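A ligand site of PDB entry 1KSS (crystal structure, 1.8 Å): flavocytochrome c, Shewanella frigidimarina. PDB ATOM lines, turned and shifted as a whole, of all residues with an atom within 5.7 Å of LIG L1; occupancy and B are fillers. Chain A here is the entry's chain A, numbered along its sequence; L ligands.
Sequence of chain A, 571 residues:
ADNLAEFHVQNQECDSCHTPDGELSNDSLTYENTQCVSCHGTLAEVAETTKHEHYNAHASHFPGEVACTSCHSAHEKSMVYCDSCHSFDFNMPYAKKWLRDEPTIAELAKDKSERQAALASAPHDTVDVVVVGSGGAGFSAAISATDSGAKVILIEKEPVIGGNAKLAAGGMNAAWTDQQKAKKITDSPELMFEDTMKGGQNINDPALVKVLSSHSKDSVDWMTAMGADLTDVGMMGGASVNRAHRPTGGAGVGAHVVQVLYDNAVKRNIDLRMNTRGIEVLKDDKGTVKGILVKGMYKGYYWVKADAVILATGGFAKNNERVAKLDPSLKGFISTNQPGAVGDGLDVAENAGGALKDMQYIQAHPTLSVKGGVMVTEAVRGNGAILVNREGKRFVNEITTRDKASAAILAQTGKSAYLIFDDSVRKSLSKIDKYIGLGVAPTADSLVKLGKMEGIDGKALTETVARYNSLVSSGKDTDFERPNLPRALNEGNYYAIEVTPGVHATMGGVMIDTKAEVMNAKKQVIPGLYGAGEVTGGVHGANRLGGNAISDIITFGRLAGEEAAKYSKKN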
ATOM      1  N   ALA A 168     -26.421  19.889  11.152  1.00  0.00           N
ATOM      2  CA  ALA A 168     -25.739  19.761   9.880  1.00  0.00           C
ATOM      3  C   ALA A 168     -26.419  18.795   8.909  1.00  0.00           C
ATOM      4  O   ALA A 168     -26.937  17.755   9.354  1.00  0.00           O
ATOM      5  CB  ALA A 168     -24.277  19.299  10.104  1.00  0.00           C
ATOM      6  N   ALA A 169     -26.445  19.146   7.626  1.00  0.00           N
ATOM      7  CA  ALA A 169     -27.132  18.310   6.658  1.00  0.00           C
ATOM      8  C   ALA A 169     -26.249  17.847   5.491  1.00  0.00           C
ATOM      9  O   ALA A 169     -26.064  16.615   5.353  1.00  0.00           O
ATOM     10  CB  ALA A 169     -28.359  19.043   6.127  1.00  0.00           C
ATOM     11  N   GLY A 170     -25.657  18.762   4.755  1.00  0.00           N
ATOM     12  CA  GLY A 170     -24.981  18.452   3.503  1.00  0.00           C
ATOM     13  C   GLY A 170     -23.834  17.473   3.523  1.00  0.00           C
ATOM     14  O   GLY A 170     -23.707  16.687   2.546  1.00  0.00           O
ATOM     15  N   GLY A 171     -22.958  17.507   4.523  1.00  0.00           N
ATOM     16  CA  GLY A 171     -21.909  16.453   4.540  1.00  0.00           C
ATOM     17  C   GLY A 171     -20.601  16.871   5.214  1.00  0.00           C
ATOM     18  O   GLY A 171     -20.460  18.002   5.644  1.00  0.00           O
ATOM     19  N   MET A 236     -20.934  19.933  -3.039  1.00  0.00           N
ATOM     20  CA  MET A 236     -21.355  21.185  -2.433  1.00  0.00           C
ATOM     21  C   MET A 236     -20.710  22.351  -3.212  1.00  0.00           C
ATOM     22  O   MET A 236     -19.921  22.074  -4.086  1.00  0.00           O
ATOM     23  CB  MET A 236     -20.920  21.278  -0.975  1.00  0.00           C
ATOM     24  CG  MET A 236     -21.447  20.057  -0.189  1.00  0.00           C
ATOM     25  SD  MET A 236     -23.224  20.400   0.083  1.00  0.00           S
ATOM     26  CE  MET A 236     -23.049  21.271   1.608  1.00  0.00           C
ATOM     27  N   GLN A 363     -20.356  34.535   7.383  1.00  0.00           N
ATOM     28  CA  GLN A 363     -21.100  33.961   6.273  1.00  0.00           C
ATOM     29  C   GLN A 363     -22.609  33.910   6.421  1.00  0.00           C
ATOM     30  O   GLN A 363     -23.193  33.480   7.425  1.00  0.00           O
ATOM     31  CB  GLN A 363     -20.603  32.478   6.102  1.00  0.00           C
ATOM     32  CG  GLN A 363     -21.375  31.736   4.979  1.00  0.00           C
ATOM     33  CD  GLN A 363     -20.662  30.424   4.659  1.00  0.00           C
ATOM     34  OE1 GLN A 363     -20.991  29.370   5.216  1.00  0.00           O
ATOM     35  NE2 GLN A 363     -19.655  30.489   3.786  1.00  0.00           N
ATOM     36  N   HIS A 365     -25.675  31.956   4.784  1.00  0.00           N
ATOM     37  CA  HIS A 365     -26.049  30.810   3.936  1.00  0.00           C
ATOM     38  C   HIS A 365     -27.078  31.344   2.927  1.00  0.00           C
ATOM     39  O   HIS A 365     -28.038  32.028   3.329  1.00  0.00           O
ATOM     40  CB  HIS A 365     -26.663  29.746   4.828  1.00  0.00           C
ATOM     41  CG  HIS A 365     -26.851  28.421   4.156  1.00  0.00           C
ATOM     42  ND1 HIS A 365     -27.717  28.168   3.135  1.00  0.00           N
ATOM     43  CD2 HIS A 365     -26.205  27.255   4.445  1.00  0.00           C
ATOM     44  CE1 HIS A 365     -27.620  26.902   2.781  1.00  0.00           C
ATOM     45  NE2 HIS A 365     -26.703  26.308   3.539  1.00  0.00           N
ATOM     46  N   MET A 375     -32.713  26.482   7.765  1.00  0.00           N
ATOM     47  CA  MET A 375     -31.814  26.234   6.662  1.00  0.00           C
ATOM     48  C   MET A 375     -32.318  25.139   5.715  1.00  0.00           C
ATOM     49  O   MET A 375     -32.789  24.133   6.231  1.00  0.00           O
ATOM     50  CB  MET A 375     -30.432  25.746   7.199  1.00  0.00           C
ATOM     51  CG  MET A 375     -29.295  25.895   6.180  1.00  0.00           C
ATOM     52  SD  MET A 375     -27.899  24.774   6.548  1.00  0.00           S
ATOM     53  CE  MET A 375     -28.846  23.234   6.436  1.00  0.00           C
ATOM     54  N   VAL A 376     -32.141  25.314   4.411  1.00  0.00           N
ATOM     55  CA  VAL A 376     -32.421  24.336   3.372  1.00  0.00           C
ATOM     56  C   VAL A 376     -31.046  23.926   2.811  1.00  0.00           C
ATOM     57  O   VAL A 376     -30.319  24.763   2.277  1.00  0.00           O
ATOM     58  CB  VAL A 376     -33.376  24.792   2.277  1.00  0.00           C
ATOM     59  CG1 VAL A 376     -33.551  23.767   1.145  1.00  0.00           C
ATOM     60  CG2 VAL A 376     -34.757  25.090   2.884  1.00  0.00           C
ATOM     61  N   THR A 377     -30.644  22.666   2.988  1.00  0.00           N
ATOM     62  CA  THR A 377     -29.277  22.287   2.582  1.00  0.00           C
ATOM     63  C   THR A 377     -28.889  22.660   1.175  1.00  0.00           C
ATOM     64  O   THR A 377     -29.570  22.529   0.162  1.00  0.00           O
ATOM     65  CB  THR A 377     -29.010  20.793   2.895  1.00  0.00           C
ATOM     66  OG1 THR A 377     -27.636  20.477   2.597  1.00  0.00           O
ATOM     67  CG2 THR A 377     -29.915  19.825   2.100  1.00  0.00           C
ATOM     68  N   GLU A 378     -27.596  23.029   1.033  1.00  0.00           N
ATOM     69  CA  GLU A 378     -26.900  23.290  -0.215  1.00  0.00           C
ATOM     70  C   GLU A 378     -26.787  21.991  -1.002  1.00  0.00           C
ATOM     71  O   GLU A 378     -26.660  21.992  -2.228  1.00  0.00           O
ATOM     72  CB  GLU A 378     -25.509  23.887   0.114  1.00  0.00           C
ATOM     73  CG  GLU A 378     -24.612  24.156  -1.076  1.00  0.00           C
ATOM     74  CD  GLU A 378     -23.596  25.251  -0.779  1.00  0.00           C
ATOM     75  OE1 GLU A 378     -24.042  26.345  -0.357  1.00  0.00           O
ATOM     76  OE2 GLU A 378     -22.392  25.025  -0.967  1.00  0.00           O
ATOM     77  N   ALA A 379     -26.970  20.825  -0.356  1.00  0.00           N
ATOM     78  CA  ALA A 379     -26.973  19.546  -1.079  1.00  0.00           C
ATOM     79  C   ALA A 379     -28.189  19.439  -1.986  1.00  0.00           C
ATOM     80  O   ALA A 379     -28.150  18.645  -2.943  1.00  0.00           O
ATOM     81  CB  ALA A 379     -26.907  18.408  -0.062  1.00  0.00           C
ATOM     82  N   ARG A 402     -20.749  30.749  -1.337  1.00  0.00           N
ATOM     83  CA  ARG A 402     -21.893  31.353  -0.642  1.00  0.00           C
ATOM     84  C   ARG A 402     -21.969  32.861  -0.660  1.00  0.00           C
ATOM     85  O   ARG A 402     -23.072  33.417  -0.685  1.00  0.00           O
ATOM     86  CB  ARG A 402     -21.964  30.805   0.798  1.00  0.00           C
ATOM     87  CG  ARG A 402     -22.298  29.299   0.707  1.00  0.00           C
ATOM     88  CD  ARG A 402     -22.143  28.637   2.070  1.00  0.00           C
ATOM     89  NE  ARG A 402     -22.692  27.276   2.054  1.00  0.00           N
ATOM     90  CZ  ARG A 402     -22.675  26.430   3.069  1.00  0.00           C
ATOM     91  NH1 ARG A 402     -22.128  26.717   4.237  1.00  0.00           N
ATOM     92  NH2 ARG A 402     -23.234  25.209   2.898  1.00  0.00           N
ATOM     93  N   HIS A 504     -25.234  32.477   9.198  1.00  0.00           N
ATOM     94  CA  HIS A 504     -24.995  31.040   9.430  1.00  0.00           C
ATOM     95  C   HIS A 504     -23.698  30.656  10.112  1.00  0.00           C
ATOM     96  O   HIS A 504     -23.688  29.730  10.963  1.00  0.00           O
ATOM     97  CB  HIS A 504     -24.988  30.427   7.988  1.00  0.00           C
ATOM     98  CG  HIS A 504     -24.818  28.919   7.941  1.00  0.00           C
ATOM     99  ND1 HIS A 504     -25.733  28.039   8.485  1.00  0.00           N
ATOM    100  CD2 HIS A 504     -23.845  28.153   7.400  1.00  0.00           C
ATOM    101  CE1 HIS A 504     -25.318  26.790   8.307  1.00  0.00           C
ATOM    102  NE2 HIS A 504     -24.173  26.818   7.617  1.00  0.00           N
ATOM    103  N   ARG A 544     -16.257  30.160   4.196  1.00  0.00           N
ATOM    104  CA  ARG A 544     -16.096  28.708   4.390  1.00  0.00           C
ATOM    105  C   ARG A 544     -16.772  27.911   3.271  1.00  0.00           C
ATOM    106  O   ARG A 544     -17.925  28.228   2.938  1.00  0.00           O
ATOM    107  CB  ARG A 544     -16.771  28.312   5.705  1.00  0.00           C
ATOM    108  CG  ARG A 544     -16.613  26.815   5.982  1.00  0.00           C
ATOM    109  CD  ARG A 544     -16.874  26.503   7.444  1.00  0.00           C
ATOM    110  NE  ARG A 544     -18.244  26.681   7.879  1.00  0.00           N
ATOM    111  CZ  ARG A 544     -19.283  26.030   7.378  1.00  0.00           C
ATOM    112  NH1 ARG A 544     -19.153  25.144   6.382  1.00  0.00           N
ATOM    113  NH2 ARG A 544     -20.463  26.253   7.930  1.00  0.00           N
ATOM    114  N   LEU A 545     -16.174  26.803   2.827  1.00  0.00           N
ATOM    115  CA  LEU A 545     -16.834  25.957   1.847  1.00  0.00           C
ATOM    116  C   LEU A 545     -17.812  24.999   2.546  1.00  0.00           C
ATOM    117  O   LEU A 545     -17.500  24.449   3.628  1.00  0.00           O
ATOM    118  CB  LEU A 545     -15.810  25.061   1.098  1.00  0.00           C
ATOM    119  CG  LEU A 545     -14.863  25.776   0.115  1.00  0.00           C
ATOM    120  CD1 LEU A 545     -13.976  24.787  -0.657  1.00  0.00           C
ATOM    121  CD2 LEU A 545     -15.596  26.669  -0.887  1.00  0.00           C
ATOM    122  N   GLY A 546     -18.949  24.733   1.897  1.00  0.00           N
ATOM    123  CA  GLY A 546     -19.910  23.781   2.495  1.00  0.00           C
ATOM    124  C   GLY A 546     -19.252  22.410   2.679  1.00  0.00           C
ATOM    125  O   GLY A 546     -18.548  22.029   1.752  1.00  0.00           O
ATOM    126  N   GLY A 547     -19.469  21.755   3.834  1.00  0.00           N
ATOM    127  CA  GLY A 547     -18.812  20.468   4.131  1.00  0.00           C
ATOM    128  C   GLY A 547     -17.507  20.590   4.901  1.00  0.00           C
ATOM    129  O   GLY A 547     -16.931  19.610   5.463  1.00  0.00           O
ATOM    130  N   ASN A 548     -16.885  21.809   4.890  1.00  0.00           N
ATOM    131  CA  ASN A 548     -15.588  21.928   5.546  1.00  0.00           C
ATOM    132  C   ASN A 548     -15.714  22.140   7.064  1.00  0.00           C
ATOM    133  O   ASN A 548     -14.700  21.877   7.749  1.00  0.00           O
ATOM    134  CB  ASN A 548     -14.707  23.045   4.926  1.00  0.00           C
ATOM    135  CG  ASN A 548     -13.775  22.607   3.807  1.00  0.00           C
ATOM    136  OD1 ASN A 548     -13.639  21.430   3.468  1.00  0.00           O
ATOM    137  ND2 ASN A 548     -13.036  23.548   3.213  1.00  0.00           N
ATOM    138  N   ALA A 549     -16.870  22.502   7.618  1.00  0.00           N
ATOM    139  CA  ALA A 549     -16.886  22.692   9.084  1.00  0.00           C
ATOM    140  C   ALA A 549     -17.000  21.366   9.843  1.00  0.00           C
ATOM    141  O   ALA A 549     -16.362  21.207  10.871  1.00  0.00           O
ATOM    142  CB  ALA A 549     -17.971  23.649   9.541  1.00  0.00           C
HETATM  143  O1  LIG L   1     -21.067  23.404   5.588  1.00  0.00           O
HETATM  144  C1  LIG L   1     -22.247  23.736   5.659  1.00  0.00           C
HETATM  145  O2  LIG L   1     -22.559  24.795   6.403  1.00  0.00           O
HETATM  146  C2  LIG L   1     -23.293  22.990   4.930  1.00  0.00           C
HETATM  147  C3  LIG L   1     -24.589  23.326   5.181  1.00  0.00           C
HETATM  148  C4  LIG L   1     -25.616  22.794   4.228  1.00  0.00           C
HETATM  149  O3  LIG L   1     -25.940  21.524   4.363  1.00  0.00           O
HETATM  150  O4  LIG L   1     -26.064  23.526   3.378  1.00  0.00           O
HETATM  151  P1  LG2 L   2     -21.331  23.486  18.163  1.00  0.00           P
HETATM  152  O1  LG2 L   2     -22.091  24.752  17.965  1.00  0.00           O
HETATM  153  O2  LG2 L   2     -21.727  22.240  17.496  1.00  0.00           O
HETATM  154  O3  LG2 L   2     -21.279  23.187  19.728  1.00  0.00           O
HETATM  155  C1  LG2 L   2     -20.806  24.098  20.746  1.00  0.00           C
HETATM  156  C2  LG2 L   2     -21.526  23.853  22.078  1.00  0.00           C
HETATM  157  O4  LG2 L   2     -20.892  24.688  23.076  1.00  0.00           O
HETATM  158  C3  LG2 L   2     -23.004  24.283  22.049  1.00  0.00           C
HETATM  159  O5  LG2 L   2     -23.872  23.242  22.405  1.00  0.00           O
HETATM  160  C4  LG2 L   2     -23.031  25.499  22.991  1.00  0.00           C
HETATM  161  O6  LG2 L   2     -24.316  25.640  23.638  1.00  0.00           O
HETATM  162  C5  LG2 L   2     -21.908  25.103  23.989  1.00  0.00           C
HETATM  163  N1  LG2 L   2     -21.459  26.271  24.748  1.00  0.00           N
HETATM  164  C6  LG2 L   2     -21.223  27.563  24.305  1.00  0.00           C
HETATM  165  N2  LG2 L   2     -20.693  28.368  25.221  1.00  0.00           N
HETATM  166  C7  LG2 L   2     -20.618  27.552  26.366  1.00  0.00           C
HETATM  167  C8  LG2 L   2     -20.163  27.754  27.667  1.00  0.00           C
HETATM  168  N3  LG2 L   2     -19.697  28.951  28.114  1.00  0.00           N
HETATM  169  N4  LG2 L   2     -20.152  26.746  28.554  1.00  0.00           N
HETATM  170  C9  LG2 L   2     -20.630  25.526  28.163  1.00  0.00           C
HETATM  171  N5  LG2 L   2     -21.107  25.210  26.925  1.00  0.00           N
HETATM  172  C10 LG2 L   2     -21.075  26.275  26.069  1.00  0.00           C
HETATM  173  N6  LG2 L   2     -20.971  22.128   8.637  1.00  0.00           N
HETATM  174  C11 LG2 L   2     -20.590  21.305   7.600  1.00  0.00           C
HETATM  175  O7  LG2 L   2     -19.454  21.186   7.188  1.00  0.00           O
HETATM  176  N7  LG2 L   2     -21.498  20.511   6.904  1.00  0.00           N
HETATM  177  C12 LG2 L   2     -22.877  20.490   7.146  1.00  0.00           C
HETATM  178  O8  LG2 L   2     -23.625  19.807   6.508  1.00  0.00           O
HETATM  179  C13 LG2 L   2     -23.308  21.627   8.001  1.00  0.00           C
HETATM  180  N8  LG2 L   2     -24.591  21.873   8.081  1.00  0.00           N
HETATM  181  C14 LG2 L   2     -24.969  22.843   9.001  1.00  0.00           C
HETATM  182  C15 LG2 L   2     -26.387  23.076   9.212  1.00  0.00           C
HETATM  183  C16 LG2 L   2     -26.810  23.995  10.187  1.00  0.00           C
HETATM  184  C17 LG2 L   2     -28.278  24.229  10.405  1.00  0.00           C
HETATM  185  C18 LG2 L   2     -25.804  24.660  10.955  1.00  0.00           C
HETATM  186  C19 LG2 L   2     -26.073  25.654  12.062  1.00  0.00           C
HETATM  187  C20 LG2 L   2     -24.414  24.479  10.726  1.00  0.00           C
HETATM  188  C21 LG2 L   2     -24.001  23.553   9.722  1.00  0.00           C
HETATM  189  N9  LG2 L   2     -22.664  23.342   9.520  1.00  0.00           N
HETATM  190  C22 LG2 L   2     -22.273  22.325   8.698  1.00  0.00           C
HETATM  191  C23 LG2 L   2     -21.629  23.957  10.434  1.00  0.00           C
HETATM  192  C24 LG2 L   2     -21.358  23.044  11.567  1.00  0.00           C
HETATM  193  O9  LG2 L   2     -22.555  22.403  12.144  1.00  0.00           O
HETATM  194  C25 LG2 L   2     -20.797  23.942  12.744  1.00  0.00           C
HETATM  195  O10 LG2 L   2     -19.523  24.471  12.301  1.00  0.00           O
HETATM  196  C26 LG2 L   2     -20.640  23.132  14.063  1.00  0.00           C
HETATM  197  O11 LG2 L   2     -20.421  21.785  13.489  1.00  0.00           O
HETATM  198  C27 LG2 L   2     -19.364  23.681  14.759  1.00  0.00           C
HETATM  199  O12 LG2 L   2     -19.278  22.664  15.736  1.00  0.00           O
HETATM  200  P2  LG2 L   2     -18.623  23.014  17.115  1.00  0.00           P
HETATM  201  O13 LG2 L   2     -18.396  21.745  17.875  1.00  0.00           O
HETATM  202  O14 LG2 L   2     -17.464  23.917  17.018  1.00  0.00           O
HETATM  203  O15 LG2 L   2     -19.792  23.847  17.848  1.00  0.00           O
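The backbone NH (N) of Gly 170 lies within hydrogen-bond range of an oxygen (O3) of LIG L1, 2.8 Å away. An oxygen (O8) of LG2 L2 sits at hydrogen-bond distance from the backbone NH of Gly 170 (2.9 Å). O3 of LIG L1 sits at hydrogen-bond distance from OG1 of Thr 377. An oxygen (O2) of LIG L1 lies within salt-bridge range of the guanidinium group (NH1) of Arg 402, 2.9 Å away. The backbone NH of Ala 549 is in hydrogen-bond range of an oxygen (O7) of LG2 L2 (2.9 Å). N of Gly 547 sits close to O7 of LG2 L2, 3.4 Å away. The backbone NH (N) of Gly 171 lies within hydrogen-bond range of an oxygen (O8) of LG2 L2 (3.1 Å). An oxygen (O8) of LG2 L2 is in hydrogen-bond range of the backbone NH of Ala 169, 3.1 Å away. The backbone carbonyl oxygen (O) of Gly 171 lies within hydrogen-bond range of a nitrogen (N7) of LG2 L2, at 3.0 Å. The backbone NH of Gly 547 sits at hydrogen-bond distance from an oxygen (O1) of LIG L1 (2.9 Å). O4 of LIG L1 is in hydrogen-bond range of N of Glu 378. A ring nitrogen (NE2) of His 504 is in hydrogen-bond range of an oxygen (O2) of LIG L1, at 2.9 Å. An oxygen (O1) of LIG L1 lies within salt-bridge range of the guanidinium group (NH1) of Arg 544 (2.7 Å). NE2 of His 365 lies within hydrogen-bond range of O4 of LIG L1 (2.9 Å).
NE of Arg 402 lies within salt-bridge range of OE1 of Glu 378 (2.9 Å). NE2 of His 365 sits at hydrogen-bond distance from SD of Met 375 (3.6 Å). The side-chain amide nitrogen (NE2) of Gln 363 lies within hydrogen-bond range of the backbone carbonyl oxygen (O) of Arg 544 (3.0 Å). OG1 of Thr 377 is in hydrogen-bond range of N of Gly 170 (3.4 Å). SD of Met 236 is in hydrogen-bond range of N of Ala 379 (3.8 Å). The guanidinium group (NH1) of Arg 402 sits at hydrogen-bond distance from the side-chain amide oxygen (OE1) of Gln 363, 3.0 Å away. OG1 of Thr 377 sits at hydrogen-bond distance from N of Ala 379 (3.0 Å). N of His 504 sits at hydrogen-bond distance from O of Gln 363.
A nitrogen (N7) of LG2 L2 lies close to an oxygen (O1) of LIG L1 (3.2 Å).
Ala 169 touches LIG L1 (C to O3, 3.9 Å). Met 236 touches LIG L1. Met 375 touches LIG L1. Gly 546 touches LIG L1 (CA to O1, 3.3 Å). 12 residues have an atom within 4 Å of LIG L1: Ala 169, Gly 170, Met 236, His 365, Met 375, Thr 377, Glu 378, Arg 402, His 504, Arg 544, Gly 546 and Gly 547. Along chain A the residues within 4 Å of LIG L1 span positions 169 to 547. The nearest printed residue that does not touch LIG L1 is Leu 545 (4.2 Å).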
